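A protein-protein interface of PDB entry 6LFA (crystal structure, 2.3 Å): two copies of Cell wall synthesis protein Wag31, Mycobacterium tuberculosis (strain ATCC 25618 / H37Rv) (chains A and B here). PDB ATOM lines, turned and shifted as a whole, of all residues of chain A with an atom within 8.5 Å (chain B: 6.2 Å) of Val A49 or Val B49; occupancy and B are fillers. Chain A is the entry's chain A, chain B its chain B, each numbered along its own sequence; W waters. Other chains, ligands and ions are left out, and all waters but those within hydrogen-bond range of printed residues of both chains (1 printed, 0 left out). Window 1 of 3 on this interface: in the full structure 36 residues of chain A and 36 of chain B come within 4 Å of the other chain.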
ATOM      1  N   LEU A  17     -26.227 -12.492   8.072  1.00  0.00           N
ATOM      2  CA  LEU A  17     -27.137 -11.947   9.081  1.00  0.00           C
ATOM      3  C   LEU A  17     -27.193 -10.438   8.883  1.00  0.00           C
ATOM      4  O   LEU A  17     -26.164  -9.751   8.974  1.00  0.00           O
ATOM      5  CB  LEU A  17     -26.699 -12.302  10.501  1.00  0.00           C
ATOM      6  CG  LEU A  17     -27.704 -11.840  11.554  1.00  0.00           C
ATOM      7  CD1 LEU A  17     -28.958 -12.730  11.527  1.00  0.00           C
ATOM      8  CD2 LEU A  17     -27.065 -11.808  12.927  1.00  0.00           C
ATOM      9  N   THR A  18     -28.376  -9.935   8.526  1.00  0.00           N
ATOM     10  CA  THR A  18     -28.594  -8.519   8.302  1.00  0.00           C
ATOM     11  C   THR A  18     -29.541  -7.947   9.351  1.00  0.00           C
ATOM     12  O   THR A  18     -30.263  -8.687  10.029  1.00  0.00           O
ATOM     13  CB  THR A  18     -29.197  -8.279   6.925  1.00  0.00           C
ATOM     14  OG1 THR A  18     -30.483  -8.902   6.905  1.00  0.00           O
ATOM     15  CG2 THR A  18     -28.300  -8.846   5.848  1.00  0.00           C
ATOM     16  N   PRO A  19     -29.570  -6.629   9.506  1.00  0.00           N
ATOM     17  CA  PRO A  19     -30.560  -6.043  10.428  1.00  0.00           C
ATOM     18  C   PRO A  19     -31.976  -6.491  10.113  1.00  0.00           C
ATOM     19  O   PRO A  19     -32.736  -6.821  11.026  1.00  0.00           O
ATOM     20  CB  PRO A  19     -30.341  -4.520  10.231  1.00  0.00           C
ATOM     21  CG  PRO A  19     -28.901  -4.414   9.875  1.00  0.00           C
ATOM     22  CD  PRO A  19     -28.708  -5.593   8.897  1.00  0.00           C
ATOM     23  N   ASP A  21     -32.943  -9.361   8.900  1.00  0.00           N
ATOM     24  CA  ASP A  21     -33.101 -10.702   9.476  1.00  0.00           C
ATOM     25  C   ASP A  21     -33.374 -10.626  10.974  1.00  0.00           C
ATOM     26  O   ASP A  21     -34.268 -11.296  11.493  1.00  0.00           O
ATOM     27  CB  ASP A  21     -31.839 -11.547   9.224  1.00  0.00           C
ATOM     28  CG  ASP A  21     -31.541 -11.752   7.736  1.00  0.00           C
ATOM     29  OD1 ASP A  21     -32.500 -11.847   6.946  1.00  0.00           O
ATOM     30  OD2 ASP A  21     -30.339 -11.849   7.360  1.00  0.00           O
ATOM     31  N   VAL A  22     -32.600  -9.820  11.696  1.00  0.00           N
ATOM     32  CA  VAL A  22     -32.829  -9.720  13.130  1.00  0.00           C
ATOM     33  C   VAL A  22     -34.247  -9.209  13.385  1.00  0.00           C
ATOM     34  O   VAL A  22     -34.976  -9.738  14.237  1.00  0.00           O
ATOM     35  CB  VAL A  22     -31.754  -8.826  13.791  1.00  0.00           C
ATOM     36  CG1 VAL A  22     -31.974  -8.760  15.296  1.00  0.00           C
ATOM     37  CG2 VAL A  22     -30.339  -9.359  13.499  1.00  0.00           C
ATOM     38  N   HIS A  23     -34.680  -8.226  12.592  1.00  0.00           N
ATOM     39  CA  HIS A  23     -35.984  -7.593  12.785  1.00  0.00           C
ATOM     40  C   HIS A  23     -37.114  -8.565  12.510  1.00  0.00           C
ATOM     41  O   HIS A  23     -38.131  -8.543  13.202  1.00  0.00           O
ATOM     42  CB  HIS A  23     -36.129  -6.369  11.858  1.00  0.00           C
ATOM     43  CG  HIS A  23     -37.349  -5.540  12.134  1.00  0.00           C
ATOM     44  ND1 HIS A  23     -37.380  -4.575  13.118  1.00  0.00           N
ATOM     45  CD2 HIS A  23     -38.579  -5.533  11.564  1.00  0.00           C
ATOM     46  CE1 HIS A  23     -38.575  -4.014  13.149  1.00  0.00           C
ATOM     47  NE2 HIS A  23     -39.320  -4.571  12.211  1.00  0.00           N
ATOM     48  N   VAL A  25     -36.874 -12.089  12.350  1.00  0.00           N
ATOM     49  CA  VAL A  25     -36.769 -13.476  12.807  1.00  0.00           C
ATOM     50  C   VAL A  25     -38.019 -13.818  13.599  1.00  0.00           C
ATOM     51  O   VAL A  25     -38.525 -13.005  14.389  1.00  0.00           O
ATOM     52  CB  VAL A  25     -35.496 -13.709  13.647  1.00  0.00           C
ATOM     53  CG1 VAL A  25     -35.588 -12.994  15.006  1.00  0.00           C
ATOM     54  CG2 VAL A  25     -35.246 -15.223  13.870  1.00  0.00           C
ATOM     55  N   PHE A  27     -39.979 -16.877  16.094  1.00  0.00           N
ATOM     56  CA  PHE A  27     -39.799 -18.013  16.992  1.00  0.00           C
ATOM     57  C   PHE A  27     -41.137 -18.670  17.236  1.00  0.00           C
ATOM     58  O   PHE A  27     -42.128 -17.984  17.485  1.00  0.00           O
ATOM     59  CB  PHE A  27     -39.231 -17.618  18.334  1.00  0.00           C
ATOM     60  CG  PHE A  27     -37.975 -16.840  18.230  1.00  0.00           C
ATOM     61  CD1 PHE A  27     -36.812 -17.453  17.827  1.00  0.00           C
ATOM     62  CD2 PHE A  27     -37.958 -15.493  18.514  1.00  0.00           C
ATOM     63  CE1 PHE A  27     -35.653 -16.746  17.709  1.00  0.00           C
ATOM     64  CE2 PHE A  27     -36.773 -14.763  18.402  1.00  0.00           C
ATOM     65  CZ  PHE A  27     -35.630 -15.398  17.989  1.00  0.00           C
ATOM     66  N   VAL A  42     -36.824 -10.862  25.255  1.00  0.00           N
ATOM     67  CA  VAL A  42     -36.153 -11.262  24.028  1.00  0.00           C
ATOM     68  C   VAL A  42     -36.359 -10.200  22.947  1.00  0.00           C
ATOM     69  O   VAL A  42     -35.397  -9.761  22.308  1.00  0.00           O
ATOM     70  CB  VAL A  42     -36.631 -12.660  23.592  1.00  0.00           C
ATOM     71  CG1 VAL A  42     -36.094 -12.983  22.226  1.00  0.00           C
ATOM     72  CG2 VAL A  42     -36.154 -13.691  24.591  1.00  0.00           C
ATOM     73  N   ASP A  43     -37.596  -9.723  22.777  1.00  0.00           N
ATOM     74  CA  ASP A  43     -37.869  -8.640  21.818  1.00  0.00           C
ATOM     75  C   ASP A  43     -36.969  -7.429  22.053  1.00  0.00           C
ATOM     76  O   ASP A  43     -36.359  -6.903  21.110  1.00  0.00           O
ATOM     77  CB  ASP A  43     -39.337  -8.203  21.902  1.00  0.00           C
ATOM     78  CG  ASP A  43     -40.306  -9.194  21.247  1.00  0.00           C
ATOM     79  OD1 ASP A  43     -39.892 -10.259  20.747  1.00  0.00           O
ATOM     80  OD2 ASP A  43     -41.517  -8.897  21.239  1.00  0.00           O
ATOM     81  N   ALA A  44     -36.892  -6.954  23.313  1.00  0.00           N
ATOM     82  CA  ALA A  44     -36.055  -5.789  23.614  1.00  0.00           C
ATOM     83  C   ALA A  44     -34.578  -6.065  23.321  1.00  0.00           C
ATOM     84  O   ALA A  44     -33.873  -5.228  22.717  1.00  0.00           O
ATOM     85  CB  ALA A  44     -36.230  -5.387  25.075  1.00  0.00           C
ATOM     86  N   PHE A  45     -34.095  -7.248  23.718  1.00  0.00           N
ATOM     87  CA  PHE A  45     -32.704  -7.586  23.435  1.00  0.00           C
ATOM     88  C   PHE A  45     -32.442  -7.612  21.924  1.00  0.00           C
ATOM     89  O   PHE A  45     -31.402  -7.124  21.462  1.00  0.00           O
ATOM     90  CB  PHE A  45     -32.330  -8.924  24.082  1.00  0.00           C
ATOM     91  CG  PHE A  45     -30.868  -9.191  24.027  1.00  0.00           C
ATOM     92  CD1 PHE A  45     -30.023  -8.546  24.899  1.00  0.00           C
ATOM     93  CD2 PHE A  45     -30.318 -10.018  23.036  1.00  0.00           C
ATOM     94  CE1 PHE A  45     -28.628  -8.737  24.840  1.00  0.00           C
ATOM     95  CE2 PHE A  45     -28.925 -10.218  22.955  1.00  0.00           C
ATOM     96  CZ  PHE A  45     -28.076  -9.572  23.867  1.00  0.00           C
ATOM     97  N   LEU A  46     -33.399  -8.120  21.131  1.00  0.00           N
ATOM     98  CA  LEU A  46     -33.158  -8.232  19.691  1.00  0.00           C
ATOM     99  C   LEU A  46     -33.220  -6.868  19.019  1.00  0.00           C
ATOM    100  O   LEU A  46     -32.562  -6.657  17.993  1.00  0.00           O
ATOM    101  CB  LEU A  46     -34.142  -9.200  19.031  1.00  0.00           C
ATOM    102  CG  LEU A  46     -33.955 -10.701  19.317  1.00  0.00           C
ATOM    103  CD1 LEU A  46     -34.972 -11.566  18.516  1.00  0.00           C
ATOM    104  CD2 LEU A  46     -32.539 -11.131  19.004  1.00  0.00           C
ATOM    105  N   ASP A  47     -33.949  -5.913  19.607  1.00  0.00           N
ATOM    106  CA  ASP A  47     -33.849  -4.536  19.122  1.00  0.00           C
ATOM    107  C   ASP A  47     -32.446  -3.987  19.337  1.00  0.00           C
ATOM    108  O   ASP A  47     -31.875  -3.333  18.451  1.00  0.00           O
ATOM    109  CB  ASP A  47     -34.887  -3.641  19.800  1.00  0.00           C
ATOM    110  CG  ASP A  47     -36.310  -3.869  19.252  1.00  0.00           C
ATOM    111  OD1 ASP A  47     -36.451  -4.315  18.091  1.00  0.00           O
ATOM    112  OD2 ASP A  47     -37.293  -3.607  19.979  1.00  0.00           O
ATOM    113  N   LEU A  48     -31.871  -4.223  20.513  1.00  0.00           N
ATOM    114  CA  LEU A  48     -30.488  -3.780  20.696  1.00  0.00           C
ATOM    115  C   LEU A  48     -29.572  -4.473  19.698  1.00  0.00           C
ATOM    116  O   LEU A  48     -28.616  -3.869  19.190  1.00  0.00           O
ATOM    117  CB  LEU A  48     -29.987  -4.083  22.115  1.00  0.00           C
ATOM    118  CG  LEU A  48     -30.779  -3.619  23.320  1.00  0.00           C
ATOM    119  CD1 LEU A  48     -30.122  -4.224  24.564  1.00  0.00           C
ATOM    120  CD2 LEU A  48     -30.803  -2.118  23.364  1.00  0.00           C
ATOM    121  N   VAL A  49     -29.819  -5.765  19.442  1.00  0.00           N
ATOM    122  CA  VAL A  49     -29.017  -6.486  18.449  1.00  0.00           C
ATOM    123  C   VAL A  49     -29.160  -5.832  17.079  1.00  0.00           C
ATOM    124  O   VAL A  49     -28.171  -5.594  16.371  1.00  0.00           O
ATOM    125  CB  VAL A  49     -29.404  -7.976  18.420  1.00  0.00           C
ATOM    126  CG1 VAL A  49     -28.747  -8.693  17.252  1.00  0.00           C
ATOM    127  CG2 VAL A  49     -28.991  -8.645  19.748  1.00  0.00           C
ATOM    128  N   GLU A  50     -30.393  -5.487  16.698  1.00  0.00           N
ATOM    129  CA  GLU A  50     -30.577  -4.884  15.388  1.00  0.00           C
ATOM    130  C   GLU A  50     -29.798  -3.584  15.307  1.00  0.00           C
ATOM    131  O   GLU A  50     -29.096  -3.336  14.325  1.00  0.00           O
ATOM    132  CB  GLU A  50     -32.059  -4.672  15.105  1.00  0.00           C
ATOM    133  CG  GLU A  50     -32.289  -4.270  13.670  1.00  0.00           C
ATOM    134  CD  GLU A  50     -33.723  -3.911  13.337  1.00  0.00           C
ATOM    135  OE1 GLU A  50     -34.676  -4.457  13.941  1.00  0.00           O
ATOM    136  OE2 GLU A  50     -33.891  -3.087  12.421  1.00  0.00           O
ATOM    137  N   ASN A  51     -29.808  -2.803  16.396  1.00  0.00           N
ATOM    138  CA  ASN A  51     -29.090  -1.528  16.384  1.00  0.00           C
ATOM    139  C   ASN A  51     -27.576  -1.730  16.275  1.00  0.00           C
ATOM    140  O   ASN A  51     -26.907  -1.064  15.478  1.00  0.00           O
ATOM    141  CB  ASN A  51     -29.434  -0.726  17.631  1.00  0.00           C
ATOM    142  CG  ASN A  51     -30.891  -0.306  17.683  1.00  0.00           C
ATOM    143  OD1 ASN A  51     -31.596  -0.277  16.666  1.00  0.00           O
ATOM    144  ND2 ASN A  51     -31.347   0.049  18.873  1.00  0.00           N
ATOM    145  N   GLU A  52     -27.013  -2.642  17.073  1.00  0.00           N
ATOM    146  CA  GLU A  52     -25.568  -2.849  17.041  1.00  0.00           C
ATOM    147  C   GLU A  52     -25.112  -3.417  15.695  1.00  0.00           C
ATOM    148  O   GLU A  52     -24.078  -2.997  15.143  1.00  0.00           O
ATOM    149  CB  GLU A  52     -25.158  -3.775  18.201  1.00  0.00           C
ATOM    150  CG  GLU A  52     -23.649  -4.101  18.306  1.00  0.00           C
ATOM    151  CD  GLU A  52     -22.766  -2.916  18.638  1.00  0.00           C
ATOM    152  OE1 GLU A  52     -23.229  -1.980  19.318  1.00  0.00           O
ATOM    153  OE2 GLU A  52     -21.592  -2.920  18.210  1.00  0.00           O
ATOM    154  N   LEU A  53     -25.869  -4.363  15.139  1.00  0.00           N
ATOM    155  CA  LEU A  53     -25.510  -4.907  13.828  1.00  0.00           C
ATOM    156  C   LEU A  53     -25.546  -3.819  12.754  1.00  0.00           C
ATOM    157  O   LEU A  53     -24.656  -3.738  11.875  1.00  0.00           O
ATOM    158  CB  LEU A  53     -26.458  -6.050  13.472  1.00  0.00           C
ATOM    159  CG  LEU A  53     -26.181  -6.722  12.140  1.00  0.00           C
ATOM    160  CD1 LEU A  53     -24.811  -7.331  12.109  1.00  0.00           C
ATOM    161  CD2 LEU A  53     -27.238  -7.773  11.862  1.00  0.00           C
ATOM    162  N   THR A  54     -26.570  -2.962  12.818  1.00  0.00           N
ATOM    163  CA  THR A  54     -26.637  -1.845  11.889  1.00  0.00           C
ATOM    164  C   THR A  54     -25.397  -0.972  12.012  1.00  0.00           C
ATOM    165  O   THR A  54     -24.750  -0.655  11.008  1.00  0.00           O
ATOM    166  CB  THR A  54     -27.916  -1.048  12.134  1.00  0.00           C
ATOM    167  OG1 THR A  54     -29.043  -1.892  11.834  1.00  0.00           O
ATOM    168  CG2 THR A  54     -27.940   0.219  11.235  1.00  0.00           C
ATOM    169  N   ARG A  55     -25.007  -0.631  13.245  1.00  0.00           N
ATOM    170  CA  ARG A  55     -23.851   0.247  13.421  1.00  0.00           C
ATOM    171  C   ARG A  55     -22.564  -0.399  12.900  1.00  0.00           C
ATOM    172  O   ARG A  55     -21.705   0.279  12.317  1.00  0.00           O
ATOM    173  CB  ARG A  55     -23.699   0.634  14.896  1.00  0.00           C
ATOM    174  CG  ARG A  55     -22.436   1.455  15.201  1.00  0.00           C
ATOM    175  CD  ARG A  55     -22.240   1.700  16.700  1.00  0.00           C
ATOM    176  NE  ARG A  55     -21.576   0.583  17.386  1.00  0.00           N
ATOM    177  CZ  ARG A  55     -20.269   0.321  17.323  1.00  0.00           C
ATOM    178  NH1 ARG A  55     -19.464   1.085  16.578  1.00  0.00           N
ATOM    179  NH2 ARG A  55     -19.763  -0.722  17.999  1.00  0.00           N
ATOM    180  N   LEU A  56     -22.390  -1.697  13.131  1.00  0.00           N
ATOM    181  CA  LEU A  56     -21.147  -2.336  12.711  1.00  0.00           C
ATOM    182  C   LEU A  56     -21.088  -2.468  11.199  1.00  0.00           C
ATOM    183  O   LEU A  56     -20.017  -2.315  10.603  1.00  0.00           O
ATOM    184  CB  LEU A  56     -20.997  -3.713  13.356  1.00  0.00           C
ATOM    185  CG  LEU A  56     -20.696  -3.823  14.850  1.00  0.00           C
ATOM    186  CD1 LEU A  56     -20.876  -5.292  15.220  1.00  0.00           C
ATOM    187  CD2 LEU A  56     -19.277  -3.322  15.245  1.00  0.00           C
ATOM    188  N   ILE A  57     -22.225  -2.760  10.556  1.00  0.00           N
ATOM    189  CA  ILE A  57     -22.251  -2.792   9.090  1.00  0.00           C
ATOM    190  C   ILE A  57     -21.990  -1.401   8.527  1.00  0.00           C
ATOM    191  O   ILE A  57     -21.307  -1.251   7.500  1.00  0.00           O
ATOM    192  CB  ILE A  57     -23.584  -3.369   8.565  1.00  0.00           C
ATOM    193  CG1 ILE A  57     -23.743  -4.822   9.013  1.00  0.00           C
ATOM    194  CG2 ILE A  57     -23.682  -3.260   7.004  1.00  0.00           C
ATOM    195  CD1 ILE A  57     -25.052  -5.394   8.566  1.00  0.00           C
ATOM    196  N   LEU B  17     -23.642  -2.768  22.500  1.00  0.00           N
ATOM    197  CA  LEU B  17     -23.835  -4.193  22.733  1.00  0.00           C
ATOM    198  C   LEU B  17     -22.602  -4.941  22.254  1.00  0.00           C
ATOM    199  O   LEU B  17     -22.156  -4.739  21.118  1.00  0.00           O
ATOM    200  CB  LEU B  17     -25.065  -4.727  21.997  1.00  0.00           C
ATOM    201  CG  LEU B  17     -25.408  -6.162  22.377  1.00  0.00           C
ATOM    202  CD1 LEU B  17     -26.106  -6.127  23.730  1.00  0.00           C
ATOM    203  CD2 LEU B  17     -26.261  -6.816  21.292  1.00  0.00           C
ATOM    204  N   VAL B  22     -24.148 -10.825  24.262  1.00  0.00           N
ATOM    205  CA  VAL B  22     -25.047 -11.796  23.664  1.00  0.00           C
ATOM    206  C   VAL B  22     -24.800 -13.151  24.280  1.00  0.00           C
ATOM    207  O   VAL B  22     -25.731 -13.919  24.540  1.00  0.00           O
ATOM    208  CB  VAL B  22     -24.852 -11.832  22.140  1.00  0.00           C
ATOM    209  CG1 VAL B  22     -25.765 -12.913  21.495  1.00  0.00           C
ATOM    210  CG2 VAL B  22     -25.085 -10.437  21.568  1.00  0.00           C
ATOM    211  N   ALA B  44     -30.089 -20.814  19.197  1.00  0.00           N
ATOM    212  CA  ALA B  44     -29.334 -20.991  17.957  1.00  0.00           C
ATOM    213  C   ALA B  44     -29.183 -19.663  17.218  1.00  0.00           C
ATOM    214  O   ALA B  44     -28.109 -19.352  16.656  1.00  0.00           O
ATOM    215  CB  ALA B  44     -30.023 -22.026  17.079  1.00  0.00           C
ATOM    216  N   PHE B  45     -30.232 -18.836  17.257  1.00  0.00           N
ATOM    217  CA  PHE B  45     -30.145 -17.552  16.581  1.00  0.00           C
ATOM    218  C   PHE B  45     -29.163 -16.613  17.295  1.00  0.00           C
ATOM    219  O   PHE B  45     -28.415 -15.865  16.646  1.00  0.00           O
ATOM    220  CB  PHE B  45     -31.541 -16.948  16.486  1.00  0.00           C
ATOM    221  CG  PHE B  45     -31.583 -15.655  15.747  1.00  0.00           C
ATOM    222  CD1 PHE B  45     -31.519 -15.630  14.366  1.00  0.00           C
ATOM    223  CD2 PHE B  45     -31.701 -14.462  16.433  1.00  0.00           C
ATOM    224  CE1 PHE B  45     -31.566 -14.429  13.674  1.00  0.00           C
ATOM    225  CE2 PHE B  45     -31.751 -13.262  15.753  1.00  0.00           C
ATOM    226  CZ  PHE B  45     -31.686 -13.242  14.380  1.00  0.00           C
ATOM    227  N   LEU B  46     -29.143 -16.642  18.628  1.00  0.00           N
ATOM    228  CA  LEU B  46     -28.200 -15.807  19.352  1.00  0.00           C
ATOM    229  C   LEU B  46     -26.775 -16.270  19.110  1.00  0.00           C
ATOM    230  O   LEU B  46     -25.854 -15.450  19.130  1.00  0.00           O
ATOM    231  CB  LEU B  46     -28.527 -15.792  20.851  1.00  0.00           C
ATOM    232  CG  LEU B  46     -29.757 -14.960  21.248  1.00  0.00           C
ATOM    233  CD1 LEU B  46     -29.863 -14.851  22.750  1.00  0.00           C
ATOM    234  CD2 LEU B  46     -29.772 -13.551  20.580  1.00  0.00           C
ATOM    235  N   ASP B  47     -26.562 -17.560  18.843  1.00  0.00           N
ATOM    236  CA  ASP B  47     -25.216 -18.007  18.502  1.00  0.00           C
ATOM    237  C   ASP B  47     -24.770 -17.422  17.163  1.00  0.00           C
ATOM    238  O   ASP B  47     -23.630 -16.951  17.024  1.00  0.00           O
ATOM    239  CB  ASP B  47     -25.161 -19.541  18.484  1.00  0.00           C
ATOM    240  CG  ASP B  47     -25.088 -20.141  19.896  1.00  0.00           C
ATOM    241  OD1 ASP B  47     -24.943 -19.362  20.864  1.00  0.00           O
ATOM    242  OD2 ASP B  47     -25.184 -21.381  20.043  1.00  0.00           O
ATOM    243  N   LEU B  48     -25.645 -17.453  16.160  1.00  0.00           N
ATOM    244  CA  LEU B  48     -25.319 -16.750  14.916  1.00  0.00           C
ATOM    245  C   LEU B  48     -25.010 -15.276  15.187  1.00  0.00           C
ATOM    246  O   LEU B  48     -24.008 -14.741  14.709  1.00  0.00           O
ATOM    247  CB  LEU B  48     -26.467 -16.878  13.912  1.00  0.00           C
ATOM    248  CG  LEU B  48     -26.277 -16.187  12.565  1.00  0.00           C
ATOM    249  CD1 LEU B  48     -24.985 -16.639  11.883  1.00  0.00           C
ATOM    250  CD2 LEU B  48     -27.488 -16.497  11.686  1.00  0.00           C
ATOM    251  N   VAL B  49     -25.863 -14.607  15.967  1.00  0.00           N
ATOM    252  CA  VAL B  49     -25.635 -13.200  16.312  1.00  0.00           C
ATOM    253  C   VAL B  49     -24.240 -13.000  16.909  1.00  0.00           C
ATOM    254  O   VAL B  49     -23.461 -12.151  16.454  1.00  0.00           O
ATOM    255  CB  VAL B  49     -26.730 -12.708  17.271  1.00  0.00           C
ATOM    256  CG1 VAL B  49     -26.394 -11.311  17.836  1.00  0.00           C
ATOM    257  CG2 VAL B  49     -28.058 -12.716  16.541  1.00  0.00           C
ATOM    258  N   GLU B  50     -23.933 -13.733  17.979  1.00  0.00           N
ATOM    259  CA  GLU B  50     -22.628 -13.601  18.627  1.00  0.00           C
ATOM    260  C   GLU B  50     -21.494 -13.786  17.627  1.00  0.00           C
ATOM    261  O   GLU B  50     -20.563 -12.969  17.577  1.00  0.00           O
ATOM    262  CB  GLU B  50     -22.499 -14.613  19.770  1.00  0.00           C
ATOM    263  CG  GLU B  50     -21.135 -14.568  20.468  1.00  0.00           C
ATOM    264  CD  GLU B  50     -21.018 -15.492  21.675  1.00  0.00           C
ATOM    265  OE1 GLU B  50     -21.994 -16.199  22.031  1.00  0.00           O
ATOM    266  OE2 GLU B  50     -19.925 -15.491  22.275  1.00  0.00           O
ATOM    267  N   ASN B  51     -21.569 -14.852  16.801  1.00  0.00           N
ATOM    268  CA  ASN B  51     -20.546 -15.085  15.784  1.00  0.00           C
ATOM    269  C   ASN B  51     -20.393 -13.897  14.834  1.00  0.00           C
ATOM    270  O   ASN B  51     -19.272 -13.517  14.464  1.00  0.00           O
ATOM    271  CB  ASN B  51     -20.867 -16.334  14.965  1.00  0.00           C
ATOM    272  CG  ASN B  51     -20.554 -17.619  15.709  1.00  0.00           C
ATOM    273  OD1 ASN B  51     -19.709 -17.634  16.594  1.00  0.00           O
ATOM    274  ND2 ASN B  51     -21.259 -18.710  15.359  1.00  0.00           N
ATOM    275  N   GLU B  52     -21.508 -13.340  14.358  1.00  0.00           N
ATOM    276  CA  GLU B  52     -21.392 -12.306  13.327  1.00  0.00           C
ATOM    277  C   GLU B  52     -20.941 -10.966  13.916  1.00  0.00           C
ATOM    278  O   GLU B  52     -20.158 -10.241  13.292  1.00  0.00           O
ATOM    279  CB  GLU B  52     -22.727 -12.154  12.573  1.00  0.00           C
ATOM    280  CG  GLU B  52     -22.871 -13.159  11.439  1.00  0.00           C
ATOM    281  CD  GLU B  52     -21.794 -12.946  10.375  1.00  0.00           C
ATOM    282  OE1 GLU B  52     -21.884 -11.958   9.620  1.00  0.00           O
ATOM    283  OE2 GLU B  52     -20.831 -13.735  10.331  1.00  0.00           O
ATOM    284  N   LEU B  53     -21.402 -10.610  15.114  1.00  0.00           N
ATOM    285  CA  LEU B  53     -20.845  -9.424  15.758  1.00  0.00           C
ATOM    286  C   LEU B  53     -19.337  -9.584  15.942  1.00  0.00           C
ATOM    287  O   LEU B  53     -18.552  -8.685  15.598  1.00  0.00           O
ATOM    288  CB  LEU B  53     -21.529  -9.168  17.106  1.00  0.00           C
ATOM    289  CG  LEU B  53     -23.024  -8.859  17.108  1.00  0.00           C
ATOM    290  CD1 LEU B  53     -23.402  -8.333  18.492  1.00  0.00           C
ATOM    291  CD2 LEU B  53     -23.432  -7.900  15.982  1.00  0.00           C
ATOM    292  N   THR B  54     -18.905 -10.739  16.464  1.00  0.00           N
ATOM    293  CA  THR B  54     -17.471 -10.941  16.664  1.00  0.00           C
ATOM    294  C   THR B  54     -16.706 -10.772  15.353  1.00  0.00           C
ATOM    295  O   THR B  54     -15.679 -10.073  15.293  1.00  0.00           O
ATOM    296  CB  THR B  54     -17.210 -12.334  17.251  1.00  0.00           C
ATOM    297  OG1 THR B  54     -17.796 -12.438  18.554  1.00  0.00           O
ATOM    298  CG2 THR B  54     -15.732 -12.591  17.341  1.00  0.00           C
HETATM  299  O   HOH W   1     -23.844 -10.819   8.472  1.00  0.00           O
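Leu A17 touches Phe B45 (CD1 to CE1, 3.8 Å). CD2 of Leu A17 touches CG2 of Val B49 (3.9 Å). Val A22 touches Phe B45. Val A25 touches Phe B45 (CG2 to CE1, 3.8 Å). Phe A45 touches Val B22. CD2 of Leu A46 touches CE2 of Phe B45, 3.97 Å away. CD2 of Leu B46 touches CD2 of Leu A46, at 3.9996 Å. CG2 of Val A49 touches CD2 of Leu B17, at 3.6 Å. CG1 of Val A49 touches CG1 of Val B49, 3.6 Å away. Leu A56 touches Leu B53 (CD1 to CD2, 3.7 Å).
Printed residues of chain A that touch a printed residue of chain B: Leu A17, Val A22, Val A25, Phe A45, Leu A46, Val A49, Glu A52 and Leu A56. Hydrophobic or aromatic side chains of chain A within 4 Å of the printed part of chain B: Leu A17, Val A25, Phe A45, Leu A46, Val A49 and Leu A56. Hydrophobic or aromatic side chains of chain B that line the printed part of chain A: Leu B17, Val B22, Phe B45, Leu B46, Val B49 and Leu B53.
Of the printed residues of chain B, Phe A45 touches Leu B17 (3.8 Å) and Val B22 (3.8 Å). Of chain B, only Leu B17 (3.6 Å) and Val B49 (3.6 Å) come within 4 Å of Val A49. Printed residues of chain B within 4 Å of Glu A52: Leu B17. Of the printed residues of chain A, Leu B17 touches Phe A45, Val A49 and Glu A52. Of chain A, only Leu A17 and Val A49 come within 4 Å of Val B49. The nearest residue of chain B that does not touch Val A49 is Val B22 (4.7 Å). The nearest residue of chain A that does not touch Val B49 is Val A22 (5.1 Å).
OE2 of Glu A52 lies within salt-bridge range of NH2 of Arg A55 (2.9 Å).
OE1 of Glu A52 lies within hydrogen-bond range of N of Leu B17, 3.3 Å away.
Val A22 touches Phe B45, and with the chains exchanged Phe A45 touches Val B22. Leu A46 touches Phe B45, but with the chains exchanged Phe A45 does not touch Leu B46 (4.2 Å). Leu A46 touches its own counterpart, Leu B46. Glu A52 touches Leu B17, but with the chains exchanged Leu A17 does not touch Glu B52 (4.03 Å). Of the 12 pairs that touch across the chains among the printed residues, 8 have their exchanged pair printed and touching as well.
Water W1 bridges the side-chain carboxylate (OE1) of Glu B52 (2.5 Å) and the backbone carbonyl oxygen (O) of Leu A17 (2.6 Å).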
